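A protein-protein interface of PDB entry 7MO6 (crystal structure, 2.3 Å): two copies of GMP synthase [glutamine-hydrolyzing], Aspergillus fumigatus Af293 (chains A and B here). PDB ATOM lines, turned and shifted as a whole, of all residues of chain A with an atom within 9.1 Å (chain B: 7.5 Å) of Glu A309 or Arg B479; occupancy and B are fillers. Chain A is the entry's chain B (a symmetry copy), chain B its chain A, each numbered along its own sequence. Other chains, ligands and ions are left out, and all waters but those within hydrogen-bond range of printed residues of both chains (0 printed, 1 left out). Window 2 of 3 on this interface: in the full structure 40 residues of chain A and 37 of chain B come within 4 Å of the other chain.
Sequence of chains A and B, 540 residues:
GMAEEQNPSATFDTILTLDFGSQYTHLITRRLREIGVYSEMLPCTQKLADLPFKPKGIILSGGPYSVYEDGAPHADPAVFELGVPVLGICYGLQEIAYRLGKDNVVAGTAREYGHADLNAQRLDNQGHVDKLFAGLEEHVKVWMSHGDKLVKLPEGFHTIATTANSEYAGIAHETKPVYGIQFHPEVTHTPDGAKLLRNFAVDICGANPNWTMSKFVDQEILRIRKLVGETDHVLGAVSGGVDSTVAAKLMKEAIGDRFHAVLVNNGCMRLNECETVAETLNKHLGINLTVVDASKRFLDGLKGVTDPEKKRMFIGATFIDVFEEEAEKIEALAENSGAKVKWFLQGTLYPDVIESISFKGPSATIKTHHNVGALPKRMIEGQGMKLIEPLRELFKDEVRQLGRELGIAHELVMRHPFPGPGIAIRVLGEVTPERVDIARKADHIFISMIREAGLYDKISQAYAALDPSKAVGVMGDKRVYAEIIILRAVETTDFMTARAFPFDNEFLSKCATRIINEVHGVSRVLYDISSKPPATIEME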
ATOM      1  N   VAL A 305       9.334  -3.476 -18.046  1.00  0.00           N
ATOM      2  CA  VAL A 305      10.394  -3.671 -19.029  1.00  0.00           C
ATOM      3  C   VAL A 305      11.009  -5.051 -18.846  1.00  0.00           C
ATOM      4  O   VAL A 305      11.848  -5.259 -17.963  1.00  0.00           O
ATOM      5  CB  VAL A 305      11.467  -2.572 -18.926  1.00  0.00           C
ATOM      6  CG1 VAL A 305      12.535  -2.779 -19.988  1.00  0.00           C
ATOM      7  CG2 VAL A 305      10.833  -1.197 -19.062  1.00  0.00           C
ATOM      8  N   THR A 306      10.593  -6.003 -19.680  1.00  0.00           N
ATOM      9  CA  THR A 306      11.137  -7.352 -19.634  1.00  0.00           C
ATOM     10  C   THR A 306      12.305  -7.545 -20.589  1.00  0.00           C
ATOM     11  O   THR A 306      13.195  -8.359 -20.313  1.00  0.00           O
ATOM     12  CB  THR A 306      10.046  -8.375 -19.963  1.00  0.00           C
ATOM     13  OG1 THR A 306       9.559  -8.142 -21.290  1.00  0.00           O
ATOM     14  CG2 THR A 306       8.892  -8.254 -18.978  1.00  0.00           C
ATOM     15  N   ASP A 307      12.322  -6.819 -21.699  1.00  0.00           N
ATOM     16  CA  ASP A 307      13.412  -6.932 -22.659  1.00  0.00           C
ATOM     17  C   ASP A 307      14.682  -6.336 -22.068  1.00  0.00           C
ATOM     18  O   ASP A 307      14.677  -5.165 -21.666  1.00  0.00           O
ATOM     19  CB  ASP A 307      13.047  -6.230 -23.961  1.00  0.00           C
ATOM     20  CG  ASP A 307      14.055  -6.487 -25.063  1.00  0.00           C
ATOM     21  OD1 ASP A 307      13.988  -7.562 -25.698  1.00  0.00           O
ATOM     22  OD2 ASP A 307      14.920  -5.616 -25.292  1.00  0.00           O
ATOM     23  N   PRO A 308      15.781  -7.091 -21.991  1.00  0.00           N
ATOM     24  CA  PRO A 308      16.998  -6.540 -21.375  1.00  0.00           C
ATOM     25  C   PRO A 308      17.627  -5.413 -22.174  1.00  0.00           C
ATOM     26  O   PRO A 308      18.247  -4.522 -21.577  1.00  0.00           O
ATOM     27  CB  PRO A 308      17.925  -7.760 -21.283  1.00  0.00           C
ATOM     28  CG  PRO A 308      17.411  -8.708 -22.321  1.00  0.00           C
ATOM     29  CD  PRO A 308      15.934  -8.500 -22.384  1.00  0.00           C
ATOM     30  N   GLU A 309      17.496  -5.420 -23.504  1.00  0.00           N
ATOM     31  CA  GLU A 309      17.998  -4.302 -24.298  1.00  0.00           C
ATOM     32  C   GLU A 309      17.220  -3.026 -24.001  1.00  0.00           C
ATOM     33  O   GLU A 309      17.813  -1.949 -23.866  1.00  0.00           O
ATOM     34  CB  GLU A 309      17.928  -4.636 -25.789  1.00  0.00           C
ATOM     35  CG  GLU A 309      19.053  -5.525 -26.295  1.00  0.00           C
ATOM     36  CD  GLU A 309      20.335  -4.756 -26.562  1.00  0.00           C
ATOM     37  OE1 GLU A 309      20.297  -3.508 -26.543  1.00  0.00           O
ATOM     38  OE2 GLU A 309      21.379  -5.401 -26.797  1.00  0.00           O
ATOM     39  N   LYS A 310      15.892  -3.128 -23.896  1.00  0.00           N
ATOM     40  CA  LYS A 310      15.088  -1.955 -23.568  1.00  0.00           C
ATOM     41  C   LYS A 310      15.326  -1.497 -22.136  1.00  0.00           C
ATOM     42  O   LYS A 310      15.123  -0.318 -21.823  1.00  0.00           O
ATOM     43  CB  LYS A 310      13.605  -2.254 -23.790  1.00  0.00           C
ATOM     44  CG  LYS A 310      13.268  -2.745 -25.187  1.00  0.00           C
ATOM     45  CD  LYS A 310      11.766  -2.902 -25.363  1.00  0.00           C
ATOM     46  CE  LYS A 310      11.421  -3.515 -26.712  1.00  0.00           C
ATOM     47  NZ  LYS A 310      11.884  -4.926 -26.819  1.00  0.00           N
ATOM     48  N   LYS A 311      15.748  -2.406 -21.256  1.00  0.00           N
ATOM     49  CA  LYS A 311      16.067  -2.017 -19.887  1.00  0.00           C
ATOM     50  C   LYS A 311      17.320  -1.155 -19.843  1.00  0.00           C
ATOM     51  O   LYS A 311      17.343  -0.107 -19.187  1.00  0.00           O
ATOM     52  CB  LYS A 311      16.233  -3.261 -19.013  1.00  0.00           C
ATOM     53  N   ARG A 312      18.375  -1.575 -20.548  1.00  0.00           N
ATOM     54  CA  ARG A 312      19.615  -0.808 -20.552  1.00  0.00           C
ATOM     55  C   ARG A 312      19.426   0.559 -21.192  1.00  0.00           C
ATOM     56  O   ARG A 312      20.123   1.514 -20.830  1.00  0.00           O
ATOM     57  CB  ARG A 312      20.713  -1.584 -21.278  1.00  0.00           C
ATOM     58  CG  ARG A 312      22.118  -1.140 -20.911  1.00  0.00           C
ATOM     59  CD  ARG A 312      22.401  -1.421 -19.446  1.00  0.00           C
ATOM     60  NE  ARG A 312      23.788  -1.147 -19.085  1.00  0.00           N
ATOM     61  CZ  ARG A 312      24.794  -1.990 -19.294  1.00  0.00           C
ATOM     62  NH1 ARG A 312      24.571  -3.163 -19.870  1.00  0.00           N
ATOM     63  NH2 ARG A 312      26.024  -1.656 -18.931  1.00  0.00           N
ATOM     64  N   MET A 313      18.498   0.675 -22.145  1.00  0.00           N
ATOM     65  CA  MET A 313      18.198   1.982 -22.720  1.00  0.00           C
ATOM     66  C   MET A 313      17.566   2.903 -21.686  1.00  0.00           C
ATOM     67  O   MET A 313      17.899   4.093 -21.620  1.00  0.00           O
ATOM     68  CB  MET A 313      17.274   1.837 -23.928  1.00  0.00           C
ATOM     69  CG  MET A 313      17.877   1.094 -25.106  1.00  0.00           C
ATOM     70  SD  MET A 313      16.872   1.285 -26.590  1.00  0.00           S
ATOM     71  CE  MET A 313      15.251   0.837 -25.973  1.00  0.00           C
ATOM     72  N   PHE A 314      16.653   2.372 -20.869  1.00  0.00           N
ATOM     73  CA  PHE A 314      15.988   3.208 -19.877  1.00  0.00           C
ATOM     74  C   PHE A 314      16.942   3.643 -18.773  1.00  0.00           C
ATOM     75  O   PHE A 314      16.794   4.745 -18.232  1.00  0.00           O
ATOM     76  CB  PHE A 314      14.790   2.474 -19.275  1.00  0.00           C
ATOM     77  CG  PHE A 314      14.063   3.267 -18.229  1.00  0.00           C
ATOM     78  CD1 PHE A 314      13.191   4.280 -18.594  1.00  0.00           C
ATOM     79  CD2 PHE A 314      14.261   3.011 -16.882  1.00  0.00           C
ATOM     80  CE1 PHE A 314      12.526   5.020 -17.635  1.00  0.00           C
ATOM     81  CE2 PHE A 314      13.597   3.747 -15.919  1.00  0.00           C
ATOM     82  CZ  PHE A 314      12.731   4.754 -16.297  1.00  0.00           C
ATOM     83  N   ILE A 315      17.917   2.803 -18.422  1.00  0.00           N
ATOM     84  CA  ILE A 315      18.869   3.179 -17.380  1.00  0.00           C
ATOM     85  C   ILE A 315      19.727   4.349 -17.843  1.00  0.00           C
ATOM     86  O   ILE A 315      19.881   5.347 -17.132  1.00  0.00           O
ATOM     87  CB  ILE A 315      19.735   1.975 -16.975  1.00  0.00           C
ATOM     88  CG1 ILE A 315      18.858   0.780 -16.599  1.00  0.00           C
ATOM     89  CG2 ILE A 315      20.633   2.352 -15.810  1.00  0.00           C
ATOM     90  CD1 ILE A 315      17.920   1.049 -15.451  1.00  0.00           C
ATOM     91  N   GLY A 316      20.296   4.244 -19.046  1.00  0.00           N
ATOM     92  CA  GLY A 316      21.152   5.310 -19.541  1.00  0.00           C
ATOM     93  C   GLY A 316      20.394   6.589 -19.835  1.00  0.00           C
ATOM     94  O   GLY A 316      20.852   7.683 -19.495  1.00  0.00           O
ATOM     95  N   ILE A 425      21.061  -4.405 -13.575  1.00  0.00           N
ATOM     96  CA  ILE A 425      21.627  -5.341 -14.539  1.00  0.00           C
ATOM     97  C   ILE A 425      21.691  -6.746 -13.952  1.00  0.00           C
ATOM     98  O   ILE A 425      21.555  -7.738 -14.679  1.00  0.00           O
ATOM     99  CB  ILE A 425      23.010  -4.844 -15.004  1.00  0.00           C
ATOM    100  CG1 ILE A 425      22.842  -3.726 -16.030  1.00  0.00           C
ATOM    101  CG2 ILE A 425      23.848  -5.975 -15.584  1.00  0.00           C
ATOM    102  CD1 ILE A 425      21.794  -4.020 -17.078  1.00  0.00           C
ATOM    103  N   GLY A 429      15.592  -9.863 -16.552  1.00  0.00           N
ATOM    104  CA  GLY A 429      14.239  -9.482 -16.905  1.00  0.00           C
ATOM    105  C   GLY A 429      13.764  -8.227 -16.203  1.00  0.00           C
ATOM    106  O   GLY A 429      14.536  -7.283 -16.013  1.00  0.00           O
ATOM    107  N   THR A 536      30.064 -13.828 -20.948  1.00  0.00           N
ATOM    108  CA  THR A 536      30.398 -12.504 -20.444  1.00  0.00           C
ATOM    109  C   THR A 536      30.492 -12.568 -18.926  1.00  0.00           C
ATOM    110  O   THR A 536      30.088 -13.550 -18.297  1.00  0.00           O
ATOM    111  CB  THR A 536      29.358 -11.452 -20.855  1.00  0.00           C
ATOM    112  OG1 THR A 536      28.174 -11.623 -20.069  1.00  0.00           O
ATOM    113  CG2 THR A 536      29.002 -11.585 -22.330  1.00  0.00           C
ATOM    114  N   GLU A 538      29.204 -10.037 -16.657  1.00  0.00           N
ATOM    115  CA  GLU A 538      27.901  -9.653 -16.139  1.00  0.00           C
ATOM    116  C   GLU A 538      26.799 -10.482 -16.801  1.00  0.00           C
ATOM    117  O   GLU A 538      27.028 -11.220 -17.763  1.00  0.00           O
ATOM    118  CB  GLU A 538      27.654  -8.161 -16.363  1.00  0.00           C
ATOM    119  CG  GLU A 538      28.523  -7.237 -15.519  1.00  0.00           C
ATOM    120  CD  GLU A 538      28.034  -7.115 -14.087  1.00  0.00           C
ATOM    121  OE1 GLU A 538      28.790  -7.481 -13.162  1.00  0.00           O
ATOM    122  OE2 GLU A 538      26.890  -6.652 -13.887  1.00  0.00           O
ATOM    123  N   MET A 539      25.583 -10.349 -16.273  1.00  0.00           N
ATOM    124  CA  MET A 539      24.445 -11.100 -16.791  1.00  0.00           C
ATOM    125  C   MET A 539      23.726 -10.382 -17.924  1.00  0.00           C
ATOM    126  O   MET A 539      23.171 -11.044 -18.809  1.00  0.00           O
ATOM    127  CB  MET A 539      23.453 -11.401 -15.665  1.00  0.00           C
ATOM    128  CG  MET A 539      24.005 -12.322 -14.592  1.00  0.00           C
ATOM    129  SD  MET A 539      24.456 -13.942 -15.241  1.00  0.00           S
ATOM    130  CE  MET A 539      25.341 -14.628 -13.844  1.00  0.00           C
ATOM    131  N   GLU A 540      23.712  -9.053 -17.918  1.00  0.00           N
ATOM    132  CA  GLU A 540      23.081  -8.292 -18.992  1.00  0.00           C
ATOM    133  C   GLU A 540      24.005  -7.186 -19.488  1.00  0.00           C
ATOM    134  O   GLU A 540      25.209  -7.211 -19.233  1.00  0.00           O
ATOM    135  CB  GLU A 540      21.749  -7.695 -18.528  1.00  0.00           C
ATOM    136  CG  GLU A 540      20.721  -8.721 -18.082  1.00  0.00           C
ATOM    137  CD  GLU A 540      19.360  -8.105 -17.816  1.00  0.00           C
ATOM    138  OE1 GLU A 540      18.341  -8.739 -18.164  1.00  0.00           O
ATOM    139  OE2 GLU A 540      19.311  -6.986 -17.265  1.00  0.00           O
ATOM    140  N   ALA B 471      20.655 -13.920 -21.147  1.00  0.00           N
ATOM    141  CA  ALA B 471      21.941 -13.431 -20.678  1.00  0.00           C
ATOM    142  C   ALA B 471      22.801 -13.062 -21.878  1.00  0.00           C
ATOM    143  O   ALA B 471      22.706 -13.681 -22.941  1.00  0.00           O
ATOM    144  CB  ALA B 471      22.658 -14.467 -19.804  1.00  0.00           C
ATOM    145  N   VAL B 472      23.641 -12.043 -21.698  1.00  0.00           N
ATOM    146  CA  VAL B 472      24.454 -11.540 -22.797  1.00  0.00           C
ATOM    147  C   VAL B 472      25.519 -12.560 -23.173  1.00  0.00           C
ATOM    148  O   VAL B 472      26.068 -13.264 -22.314  1.00  0.00           O
ATOM    149  CB  VAL B 472      25.091 -10.190 -22.431  1.00  0.00           C
ATOM    150  CG1 VAL B 472      24.112  -9.067 -22.661  1.00  0.00           C
ATOM    151  CG2 VAL B 472      25.548 -10.197 -20.987  1.00  0.00           C
ATOM    152  N   GLY B 473      25.807 -12.644 -24.472  1.00  0.00           N
ATOM    153  CA  GLY B 473      26.885 -13.464 -24.980  1.00  0.00           C
ATOM    154  C   GLY B 473      27.627 -12.726 -26.077  1.00  0.00           C
ATOM    155  O   GLY B 473      27.251 -11.619 -26.468  1.00  0.00           O
ATOM    156  N   VAL B 474      28.687 -13.358 -26.570  1.00  0.00           N
ATOM    157  CA  VAL B 474      29.540 -12.777 -27.599  1.00  0.00           C
ATOM    158  C   VAL B 474      29.538 -13.717 -28.797  1.00  0.00           C
ATOM    159  O   VAL B 474      30.072 -14.833 -28.720  1.00  0.00           O
ATOM    160  CB  VAL B 474      30.968 -12.528 -27.095  1.00  0.00           C
ATOM    161  N   MET B 475      28.937 -13.274 -29.897  1.00  0.00           N
ATOM    162  CA  MET B 475      28.980 -13.980 -31.176  1.00  0.00           C
ATOM    163  C   MET B 475      29.906 -13.179 -32.087  1.00  0.00           C
ATOM    164  O   MET B 475      29.494 -12.180 -32.683  1.00  0.00           O
ATOM    165  CB  MET B 475      27.586 -14.130 -31.775  1.00  0.00           C
ATOM    166  CG  MET B 475      27.552 -14.933 -33.066  1.00  0.00           C
ATOM    167  SD  MET B 475      27.941 -16.677 -32.816  1.00  0.00           S
ATOM    168  CE  MET B 475      26.449 -17.244 -32.005  1.00  0.00           C
ATOM    169  N   GLY B 476      31.157 -13.619 -32.191  1.00  0.00           N
ATOM    170  CA  GLY B 476      32.170 -12.827 -32.856  1.00  0.00           C
ATOM    171  C   GLY B 476      32.554 -11.640 -32.000  1.00  0.00           C
ATOM    172  O   GLY B 476      33.432 -11.745 -31.138  1.00  0.00           O
ATOM    173  N   ASP B 477      31.893 -10.497 -32.224  1.00  0.00           N
ATOM    174  CA  ASP B 477      32.041  -9.353 -31.331  1.00  0.00           C
ATOM    175  C   ASP B 477      30.749  -8.546 -31.245  1.00  0.00           C
ATOM    176  O   ASP B 477      30.785  -7.349 -30.939  1.00  0.00           O
ATOM    177  CB  ASP B 477      33.213  -8.457 -31.763  1.00  0.00           C
ATOM    178  CG  ASP B 477      33.292  -8.275 -33.265  1.00  0.00           C
ATOM    179  OD1 ASP B 477      32.294  -8.565 -33.958  1.00  0.00           O
ATOM    180  OD2 ASP B 477      34.360  -7.849 -33.754  1.00  0.00           O
ATOM    181  N   LYS B 478      29.611  -9.183 -31.508  1.00  0.00           N
ATOM    182  CA  LYS B 478      28.296  -8.576 -31.359  1.00  0.00           C
ATOM    183  C   LYS B 478      27.583  -9.229 -30.183  1.00  0.00           C
ATOM    184  O   LYS B 478      27.525 -10.461 -30.094  1.00  0.00           O
ATOM    185  CB  LYS B 478      27.470  -8.735 -32.638  1.00  0.00           C
ATOM    186  N   ARG B 479      27.048  -8.407 -29.284  1.00  0.00           N
ATOM    187  CA  ARG B 479      26.382  -8.929 -28.099  1.00  0.00           C
ATOM    188  C   ARG B 479      25.039  -9.547 -28.474  1.00  0.00           C
ATOM    189  O   ARG B 479      24.245  -8.945 -29.204  1.00  0.00           O
ATOM    190  CB  ARG B 479      26.198  -7.821 -27.058  1.00  0.00           C
ATOM    191  CG  ARG B 479      25.497  -6.576 -27.580  1.00  0.00           C
ATOM    192  CD  ARG B 479      25.618  -5.392 -26.624  1.00  0.00           C
ATOM    193  NE  ARG B 479      24.980  -5.625 -25.331  1.00  0.00           N
ATOM    194  CZ  ARG B 479      25.640  -5.755 -24.184  1.00  0.00           C
ATOM    195  NH1 ARG B 479      26.963  -5.670 -24.166  1.00  0.00           N
ATOM    196  NH2 ARG B 479      24.978  -5.959 -23.052  1.00  0.00           N
ATOM    197  N   VAL B 480      24.792 -10.761 -27.982  1.00  0.00           N
ATOM    198  CA  VAL B 480      23.561 -11.486 -28.257  1.00  0.00           C
ATOM    199  C   VAL B 480      22.931 -11.901 -26.936  1.00  0.00           C
ATOM    200  O   VAL B 480      23.585 -11.945 -25.893  1.00  0.00           O
ATOM    201  CB  VAL B 480      23.794 -12.724 -29.151  1.00  0.00           C
ATOM    202  N   TYR B 481      21.637 -12.208 -26.996  1.00  0.00           N
ATOM    203  CA  TYR B 481      20.876 -12.665 -25.837  1.00  0.00           C
ATOM    204  C   TYR B 481      20.335 -14.055 -26.137  1.00  0.00           C
ATOM    205  O   TYR B 481      19.471 -14.217 -27.006  1.00  0.00           O
ATOM    206  CB  TYR B 481      19.743 -11.696 -25.502  1.00  0.00           C
ATOM    207  CG  TYR B 481      20.207 -10.417 -24.849  1.00  0.00           C
ATOM    208  CD1 TYR B 481      20.544  -9.306 -25.613  1.00  0.00           C
ATOM    209  CD2 TYR B 481      20.311 -10.319 -23.469  1.00  0.00           C
ATOM    210  CE1 TYR B 481      20.970  -8.134 -25.018  1.00  0.00           C
ATOM    211  CE2 TYR B 481      20.733  -9.152 -22.867  1.00  0.00           C
ATOM    212  CZ  TYR B 481      21.060  -8.061 -23.645  1.00  0.00           C
ATOM    213  OH  TYR B 481      21.485  -6.898 -23.047  1.00  0.00           O
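Of the 18 printed residues of chain A, 6 touch a printed residue of chain B.
Hydrophobic or aromatic side chains of chain A that line the printed part of chain B: Pro A308.
Printed residues of chain B that touch a printed residue of chain A: Ala B471, Val B472, Gly B473, Arg B479 and Tyr B481.
Hydrophobic or aromatic side chains of chain B that line the printed part of chain A: Ala B471, Val B472 and Tyr B481.
Among the printed residues, 10 pairs touch across the chains.
Among the printed residues, Asp or Glu carboxylates within 4 Å of a Lys or Arg side-chain nitrogen of the other chain: Glu A309 with Arg B479 (3.9 Å).
The backbone NH of Val B472 lies within hydrogen-bond range of the backbone carbonyl oxygen of Met A539 (3.1 Å).
O of Val B472 sits close to OG1 of Thr A536 (3.5 Å).
OE2 of Glu A309 is in salt-bridge range of NE of Arg B479.
No position is printed for both chains.
Of the 10 pairs that touch across the chains among the printed residues, none has its exchanged pair printed and touching as well.
Of the printed residues of chain B, Glu A309 touches Arg B479 (3.9 Å) and Tyr B481 (3.3 Å).
Lys B478 touches none of the printed residues of chain A.
Of the printed residues of chain B, Glu A540 touches Val B472 (3.5 Å) and Arg B479 (3.9 Å).
Of the printed residues of chain A, Gly B473 touches Thr A536 (3.9 Å).
Of the printed residues of chain B, Met A539 touches Ala B471 (3.3 Å) and Val B472 (3.1 Å).
The nearest residue of chain B that does not touch Glu A309 is Val B472 (6.2 Å).
The nearest residue of chain A that does not touch Arg B479 is Arg A312 (4.3 Å).
The nearest printed residue of chain A that does not touch Tyr B481 is Glu A540 (4.4 Å).
OD2 of Asp A307 is in hydrogen-bond range of N of Glu A309.
OG1 of Thr A536 is in hydrogen-bond range of O of Glu A538 (2.6 Å).
OE1 of Glu A540 sits at hydrogen-bond distance from N of Gly A429, at 3.4 Å.
The backbone carbonyl oxygen (O) of Val B480 is in hydrogen-bond range of the backbone NH (N) of Gly B473.
CG of Pro A308 touches CE2 of Tyr B481, at 3.4 Å.
OE2 of Glu A309 touches CE1 of Tyr B481, at 3.3 Å.
CG2 of Thr A536 touches CA of Gly B473, at 3.9 Å.
O of Glu A538 touches CG2 of Val B472 (3.7 Å).
Ala B471 touches Met A539 (CA to O, 3.3 Å).
O of Glu A540 touches CG2 of Val B472, at 3.5 Å.
C of Glu A540 touches NH2 of Arg B479, 3.9 Å away.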
